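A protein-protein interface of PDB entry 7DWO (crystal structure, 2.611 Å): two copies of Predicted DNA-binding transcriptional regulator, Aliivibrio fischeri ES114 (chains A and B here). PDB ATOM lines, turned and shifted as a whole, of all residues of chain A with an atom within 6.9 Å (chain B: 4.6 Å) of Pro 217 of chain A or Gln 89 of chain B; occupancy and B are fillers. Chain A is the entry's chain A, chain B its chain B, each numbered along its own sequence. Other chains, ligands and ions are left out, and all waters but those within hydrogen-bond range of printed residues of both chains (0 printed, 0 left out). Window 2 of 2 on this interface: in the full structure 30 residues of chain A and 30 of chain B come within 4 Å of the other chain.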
ATOM      1  N   VAL A 191       9.716 -23.705  23.365  1.00  0.00           N
ATOM      2  CA  VAL A 191       9.769 -22.775  22.244  1.00  0.00           C
ATOM      3  C   VAL A 191      11.222 -22.439  21.936  1.00  0.00           C
ATOM      4  O   VAL A 191      12.024 -22.244  22.865  1.00  0.00           O
ATOM      5  CB  VAL A 191       8.956 -21.506  22.548  1.00  0.00           C
ATOM      6  CG1 VAL A 191       8.927 -20.586  21.342  1.00  0.00           C
ATOM      7  CG2 VAL A 191       7.543 -21.874  22.981  1.00  0.00           C
ATOM      8  N   PRO A 192      11.613 -22.389  20.662  1.00  0.00           N
ATOM      9  CA  PRO A 192      12.948 -21.886  20.320  1.00  0.00           C
ATOM     10  C   PRO A 192      13.088 -20.436  20.755  1.00  0.00           C
ATOM     11  O   PRO A 192      12.248 -19.591  20.440  1.00  0.00           O
ATOM     12  CB  PRO A 192      13.005 -22.031  18.794  1.00  0.00           C
ATOM     13  CG  PRO A 192      11.972 -23.053  18.465  1.00  0.00           C
ATOM     14  CD  PRO A 192      10.882 -22.869  19.476  1.00  0.00           C
ATOM     15  N   TRP A 193      14.166 -20.148  21.479  1.00  0.00           N
ATOM     16  CA  TRP A 193      14.345 -18.865  22.140  1.00  0.00           C
ATOM     17  C   TRP A 193      15.593 -18.193  21.590  1.00  0.00           C
ATOM     18  O   TRP A 193      16.676 -18.793  21.588  1.00  0.00           O
ATOM     19  CB  TRP A 193      14.448 -19.060  23.654  1.00  0.00           C
ATOM     20  CG  TRP A 193      14.586 -17.801  24.437  1.00  0.00           C
ATOM     21  CD1 TRP A 193      14.156 -16.556  24.083  1.00  0.00           C
ATOM     22  CD2 TRP A 193      15.210 -17.662  25.718  1.00  0.00           C
ATOM     23  NE1 TRP A 193      14.470 -15.651  25.068  1.00  0.00           N
ATOM     24  CE2 TRP A 193      15.118 -16.305  26.082  1.00  0.00           C
ATOM     25  CE3 TRP A 193      15.838 -18.555  26.591  1.00  0.00           C
ATOM     26  CZ2 TRP A 193      15.631 -15.819  27.283  1.00  0.00           C
ATOM     27  CZ3 TRP A 193      16.345 -18.072  27.783  1.00  0.00           C
ATOM     28  CH2 TRP A 193      16.239 -16.716  28.118  1.00  0.00           C
ATOM     29  N   LEU A 194      15.432 -16.961  21.112  1.00  0.00           N
ATOM     30  CA  LEU A 194      16.539 -16.114  20.686  1.00  0.00           C
ATOM     31  C   LEU A 194      16.821 -15.139  21.822  1.00  0.00           C
ATOM     32  O   LEU A 194      16.062 -14.190  22.036  1.00  0.00           O
ATOM     33  CB  LEU A 194      16.194 -15.378  19.395  1.00  0.00           C
ATOM     34  CG  LEU A 194      15.521 -16.226  18.314  1.00  0.00           C
ATOM     35  CD1 LEU A 194      15.107 -15.352  17.148  1.00  0.00           C
ATOM     36  CD2 LEU A 194      16.434 -17.350  17.851  1.00  0.00           C
ATOM     37  N   THR A 195      17.904 -15.379  22.553  1.00  0.00           N
ATOM     38  CA  THR A 195      18.157 -14.685  23.804  1.00  0.00           C
ATOM     39  C   THR A 195      19.274 -13.664  23.649  1.00  0.00           C
ATOM     40  O   THR A 195      20.105 -13.738  22.739  1.00  0.00           O
ATOM     41  CB  THR A 195      18.515 -15.680  24.915  1.00  0.00           C
ATOM     42  OG1 THR A 195      18.675 -14.980  26.154  1.00  0.00           O
ATOM     43  CG2 THR A 195      19.808 -16.408  24.581  1.00  0.00           C
ATOM     44  N   TYR A 196      19.274 -12.692  24.555  1.00  0.00           N
ATOM     45  CA  TYR A 196      20.388 -11.775  24.705  1.00  0.00           C
ATOM     46  C   TYR A 196      21.428 -12.383  25.639  1.00  0.00           C
ATOM     47  O   TYR A 196      21.223 -13.439  26.241  1.00  0.00           O
ATOM     48  CB  TYR A 196      19.918 -10.430  25.260  1.00  0.00           C
ATOM     49  CG  TYR A 196      18.906  -9.712  24.403  1.00  0.00           C
ATOM     50  CD1 TYR A 196      19.290  -8.681  23.556  1.00  0.00           C
ATOM     51  CD2 TYR A 196      17.562 -10.058  24.445  1.00  0.00           C
ATOM     52  CE1 TYR A 196      18.368  -8.020  22.773  1.00  0.00           C
ATOM     53  CE2 TYR A 196      16.634  -9.405  23.664  1.00  0.00           C
ATOM     54  CZ  TYR A 196      17.040  -8.386  22.831  1.00  0.00           C
ATOM     55  OH  TYR A 196      16.117  -7.730  22.051  1.00  0.00           O
ATOM     56  N   SER A 198      22.918 -12.664  29.077  1.00  0.00           N
ATOM     57  CA  SER A 198      22.300 -12.392  30.376  1.00  0.00           C
ATOM     58  C   SER A 198      23.096 -11.401  31.215  1.00  0.00           C
ATOM     59  O   SER A 198      22.713 -11.148  32.364  1.00  0.00           O
ATOM     60  CB  SER A 198      22.103 -13.690  31.159  1.00  0.00           C
ATOM     61  OG  SER A 198      23.343 -14.254  31.542  1.00  0.00           O
ATOM     62  N   ARG A 210      12.195 -15.647  33.438  1.00  0.00           N
ATOM     63  CA  ARG A 210      12.597 -16.842  32.699  1.00  0.00           C
ATOM     64  C   ARG A 210      12.085 -18.107  33.376  1.00  0.00           C
ATOM     65  O   ARG A 210      11.549 -19.000  32.709  1.00  0.00           O
ATOM     66  CB  ARG A 210      14.118 -16.884  32.542  1.00  0.00           C
ATOM     67  CG  ARG A 210      14.645 -18.270  32.199  1.00  0.00           C
ATOM     68  CD  ARG A 210      16.109 -18.278  31.769  1.00  0.00           C
ATOM     69  NE  ARG A 210      16.568 -19.652  31.575  1.00  0.00           N
ATOM     70  CZ  ARG A 210      17.591 -20.015  30.808  1.00  0.00           C
ATOM     71  NH1 ARG A 210      18.283 -19.105  30.139  1.00  0.00           N
ATOM     72  NH2 ARG A 210      17.915 -21.297  30.703  1.00  0.00           N
ATOM     73  N   LEU A 215      11.514 -22.343  27.754  1.00  0.00           N
ATOM     74  CA  LEU A 215      12.163 -21.925  26.520  1.00  0.00           C
ATOM     75  C   LEU A 215      13.462 -22.695  26.343  1.00  0.00           C
ATOM     76  O   LEU A 215      14.130 -23.045  27.319  1.00  0.00           O
ATOM     77  CB  LEU A 215      12.473 -20.421  26.521  1.00  0.00           C
ATOM     78  CG  LEU A 215      11.396 -19.460  27.024  1.00  0.00           C
ATOM     79  CD1 LEU A 215      12.023 -18.150  27.471  1.00  0.00           C
ATOM     80  CD2 LEU A 215      10.351 -19.219  25.948  1.00  0.00           C
ATOM     81  N   THR A 216      13.823 -22.950  25.087  1.00  0.00           N
ATOM     82  CA  THR A 216      15.116 -23.552  24.784  1.00  0.00           C
ATOM     83  C   THR A 216      15.983 -22.523  24.075  1.00  0.00           C
ATOM     84  O   THR A 216      15.670 -22.142  22.936  1.00  0.00           O
ATOM     85  CB  THR A 216      14.954 -24.801  23.917  1.00  0.00           C
ATOM     86  OG1 THR A 216      13.965 -24.562  22.908  1.00  0.00           O
ATOM     87  CG2 THR A 216      14.545 -25.997  24.770  1.00  0.00           C
ATOM     88  N   PRO A 217      17.060 -22.027  24.704  1.00  0.00           N
ATOM     89  CA  PRO A 217      17.916 -21.041  24.029  1.00  0.00           C
ATOM     90  C   PRO A 217      18.637 -21.650  22.840  1.00  0.00           C
ATOM     91  O   PRO A 217      19.575 -22.433  23.017  1.00  0.00           O
ATOM     92  CB  PRO A 217      18.908 -20.617  25.124  1.00  0.00           C
ATOM     93  CG  PRO A 217      18.322 -21.108  26.415  1.00  0.00           C
ATOM     94  CD  PRO A 217      17.525 -22.322  26.068  1.00  0.00           C
ATOM     95  N   ILE A 218      18.207 -21.309  21.623  1.00  0.00           N
ATOM     96  CA  ILE A 218      18.838 -21.859  20.426  1.00  0.00           C
ATOM     97  C   ILE A 218      19.799 -20.880  19.773  1.00  0.00           C
ATOM     98  O   ILE A 218      20.555 -21.279  18.872  1.00  0.00           O
ATOM     99  CB  ILE A 218      17.787 -22.315  19.392  1.00  0.00           C
ATOM    100  CG1 ILE A 218      17.072 -21.104  18.794  1.00  0.00           C
ATOM    101  CG2 ILE A 218      16.792 -23.271  20.033  1.00  0.00           C
ATOM    102  CD1 ILE A 218      16.349 -21.403  17.503  1.00  0.00           C
ATOM    103  N   PHE A 219      19.798 -19.619  20.197  1.00  0.00           N
ATOM    104  CA  PHE A 219      20.647 -18.594  19.611  1.00  0.00           C
ATOM    105  C   PHE A 219      20.813 -17.480  20.632  1.00  0.00           C
ATOM    106  O   PHE A 219      19.873 -17.163  21.366  1.00  0.00           O
ATOM    107  CB  PHE A 219      20.041 -18.053  18.309  1.00  0.00           C
ATOM    108  CG  PHE A 219      20.852 -16.963  17.664  1.00  0.00           C
ATOM    109  CD1 PHE A 219      21.817 -17.268  16.719  1.00  0.00           C
ATOM    110  CD2 PHE A 219      20.641 -15.633  17.992  1.00  0.00           C
ATOM    111  CE1 PHE A 219      22.561 -16.270  16.121  1.00  0.00           C
ATOM    112  CE2 PHE A 219      21.384 -14.633  17.400  1.00  0.00           C
ATOM    113  CZ  PHE A 219      22.343 -14.951  16.462  1.00  0.00           C
ATOM    114  N   SER A 220      22.005 -16.892  20.672  1.00  0.00           N
ATOM    115  CA  SER A 220      22.308 -15.808  21.594  1.00  0.00           C
ATOM    116  C   SER A 220      22.996 -14.676  20.851  1.00  0.00           C
ATOM    117  O   SER A 220      23.837 -14.914  19.979  1.00  0.00           O
ATOM    118  CB  SER A 220      23.198 -16.289  22.745  1.00  0.00           C
ATOM    119  OG  SER A 220      23.516 -15.224  23.624  1.00  0.00           O
ATOM    120  N   SER B  85      27.824 -18.705  32.744  1.00  0.00           N
ATOM    121  CA  SER B  85      26.362 -18.694  32.755  1.00  0.00           C
ATOM    122  C   SER B  85      25.770 -18.714  31.347  1.00  0.00           C
ATOM    123  O   SER B  85      24.930 -19.563  31.013  1.00  0.00           O
ATOM    124  CB  SER B  85      25.890 -17.454  33.509  1.00  0.00           C
ATOM    125  OG  SER B  85      26.556 -16.298  33.022  1.00  0.00           O
ATOM    126  N   ASP B  86      26.185 -17.759  30.512  1.00  0.00           N
ATOM    127  CA  ASP B  86      25.635 -17.675  29.164  1.00  0.00           C
ATOM    128  C   ASP B  86      26.076 -18.849  28.301  1.00  0.00           C
ATOM    129  O   ASP B  86      25.306 -19.316  27.458  1.00  0.00           O
ATOM    130  CB  ASP B  86      26.027 -16.345  28.519  1.00  0.00           C
ATOM    131  CG  ASP B  86      25.286 -15.170  29.129  1.00  0.00           C
ATOM    132  OD1 ASP B  86      24.342 -15.417  29.907  1.00  0.00           O
ATOM    133  OD2 ASP B  86      25.640 -14.006  28.843  1.00  0.00           O
ATOM    134  N   LEU B  87      27.292 -19.355  28.505  1.00  0.00           N
ATOM    135  CA  LEU B  87      27.753 -20.491  27.715  1.00  0.00           C
ATOM    136  C   LEU B  87      27.057 -21.778  28.142  1.00  0.00           C
ATOM    137  O   LEU B  87      26.737 -22.626  27.301  1.00  0.00           O
ATOM    138  CB  LEU B  87      29.272 -20.628  27.829  1.00  0.00           C
ATOM    139  CG  LEU B  87      30.103 -19.524  27.181  1.00  0.00           C
ATOM    140  CD1 LEU B  87      31.582 -19.732  27.463  1.00  0.00           C
ATOM    141  CD2 LEU B  87      29.849 -19.469  25.683  1.00  0.00           C
ATOM    142  N   SER B  88      26.800 -21.933  29.441  1.00  0.00           N
ATOM    143  CA  SER B  88      26.140 -23.129  29.941  1.00  0.00           C
ATOM    144  C   SER B  88      24.680 -23.164  29.525  1.00  0.00           C
ATOM    145  O   SER B  88      24.147 -24.236  29.219  1.00  0.00           O
ATOM    146  CB  SER B  88      26.269 -23.206  31.464  1.00  0.00           C
ATOM    147  OG  SER B  88      25.802 -22.030  32.104  1.00  0.00           O
ATOM    148  N   GLN B  89      24.014 -22.008  29.509  1.00  0.00           N
ATOM    149  CA  GLN B  89      22.618 -21.996  29.082  1.00  0.00           C
ATOM    150  C   GLN B  89      22.464 -22.445  27.634  1.00  0.00           C
ATOM    151  O   GLN B  89      21.471 -23.089  27.291  1.00  0.00           O
ATOM    152  CB  GLN B  89      22.023 -20.605  29.268  1.00  0.00           C
ATOM    153  CG  GLN B  89      21.877 -20.199  30.720  1.00  0.00           C
ATOM    154  CD  GLN B  89      21.157 -18.880  30.882  1.00  0.00           C
ATOM    155  OE1 GLN B  89      20.410 -18.459  29.999  1.00  0.00           O
ATOM    156  NE2 GLN B  89      21.372 -18.220  32.013  1.00  0.00           N
ATOM    157  N   LEU B  90      23.432 -22.131  26.779  1.00  0.00           N
ATOM    158  CA  LEU B  90      23.369 -22.509  25.373  1.00  0.00           C
ATOM    159  C   LEU B  90      23.818 -23.944  25.127  1.00  0.00           C
ATOM    160  O   LEU B  90      23.509 -24.499  24.067  1.00  0.00           O
ATOM    161  CB  LEU B  90      24.228 -21.557  24.534  1.00  0.00           C
ATOM    162  CG  LEU B  90      23.854 -20.078  24.634  1.00  0.00           C
ATOM    163  CD1 LEU B  90      24.880 -19.209  23.928  1.00  0.00           C
ATOM    164  CD2 LEU B  90      22.465 -19.843  24.065  1.00  0.00           C
ATOM    165  N   GLY B  91      24.541 -24.547  26.066  1.00  0.00           N
ATOM    166  CA  GLY B  91      24.958 -25.929  25.952  1.00  0.00           C
ATOM    167  C   GLY B  91      26.389 -26.068  25.464  1.00  0.00           C
ATOM    168  O   GLY B  91      27.066 -25.101  25.108  1.00  0.00           O
ATOM    169  N   ILE B 123      24.998 -24.028  18.297  1.00  0.00           N
ATOM    170  CA  ILE B 123      24.218 -22.960  18.911  1.00  0.00           C
ATOM    171  C   ILE B 123      25.072 -21.703  18.848  1.00  0.00           C
ATOM    172  O   ILE B 123      26.081 -21.592  19.554  1.00  0.00           O
ATOM    173  CB  ILE B 123      23.821 -23.294  20.355  1.00  0.00           C
ATOM    174  CG1 ILE B 123      23.052 -24.615  20.407  1.00  0.00           C
ATOM    175  CG2 ILE B 123      22.999 -22.164  20.955  1.00  0.00           C
ATOM    176  CD1 ILE B 123      21.805 -24.627  19.556  1.00  0.00           C
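The backbone NH (N) of Ser 198 of chain A sits at hydrogen-bond distance from the side-chain carboxylate (OD2) of Asp 86 of chain B (3.0 Å).
The side-chain amide oxygen (OE1) of Gln 89 of chain B lies close to the guanidinium group (NH1) of Arg 210 of chain A (2.2 Å).
The backbone carbonyl oxygen (O) of Trp 193 of chain A lies within hydrogen-bond range of the backbone NH (N) of Ile 218 of chain A (2.9 Å).
Among the printed residues, pairs that only touch across the chains: Ile 218 of chain A with Ile 123 of chain B, Ser 220 of chain A with Leu 90 of chain B, Pro 217 of chain A with Leu 90 of chain B and Pro 217 of chain A with Gln 89 of chain B.
Printed residues of chain B within 4 Å of Pro 217 of chain A: Gln 89 and Leu 90.
Gln 89 of chain B touches two residues of chain A.
Printed residues of chain B within 4 Å of Ser 220 of chain A: Leu 90.
Printed residues of chain B within 4 Å of Arg 210 of chain A: Gln 89.
Of the printed residues of chain B, Ser 198 of chain A touches Asp 86.
Printed residues of chain A within 4 Å of Asp 86 of chain B: Ser 198.
The nearest printed residue of chain B that does not touch Pro 217 of chain A is Ile 123 of chain B (4.01 Å).
The nearest residue of chain A that does not touch Gln 89 of chain B is Ser 198 of chain A (4.5 Å).
The nearest printed residue of chain A that does not touch Leu 90 of chain B is Thr 195 of chain A (4.4 Å).
Hydrophobic or aromatic side chains of chain B within 4 Å of the printed part of chain A: Leu 90 and Ile 123.
Along chain B the printed residues that touch a printed residue of chain A span positions 86 to 123.
Hydrophobic or aromatic side chains of chain A that line the printed part of chain B: Pro 217.
Among the printed residues, no Asp or Glu carboxylate lies within 4 Å of a Lys or Arg side-chain nitrogen of the other chain.
No position is printed for both chains.
Of the 6 pairs that touch across the chains among the printed residues, none has its exchanged pair printed and touching as well.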
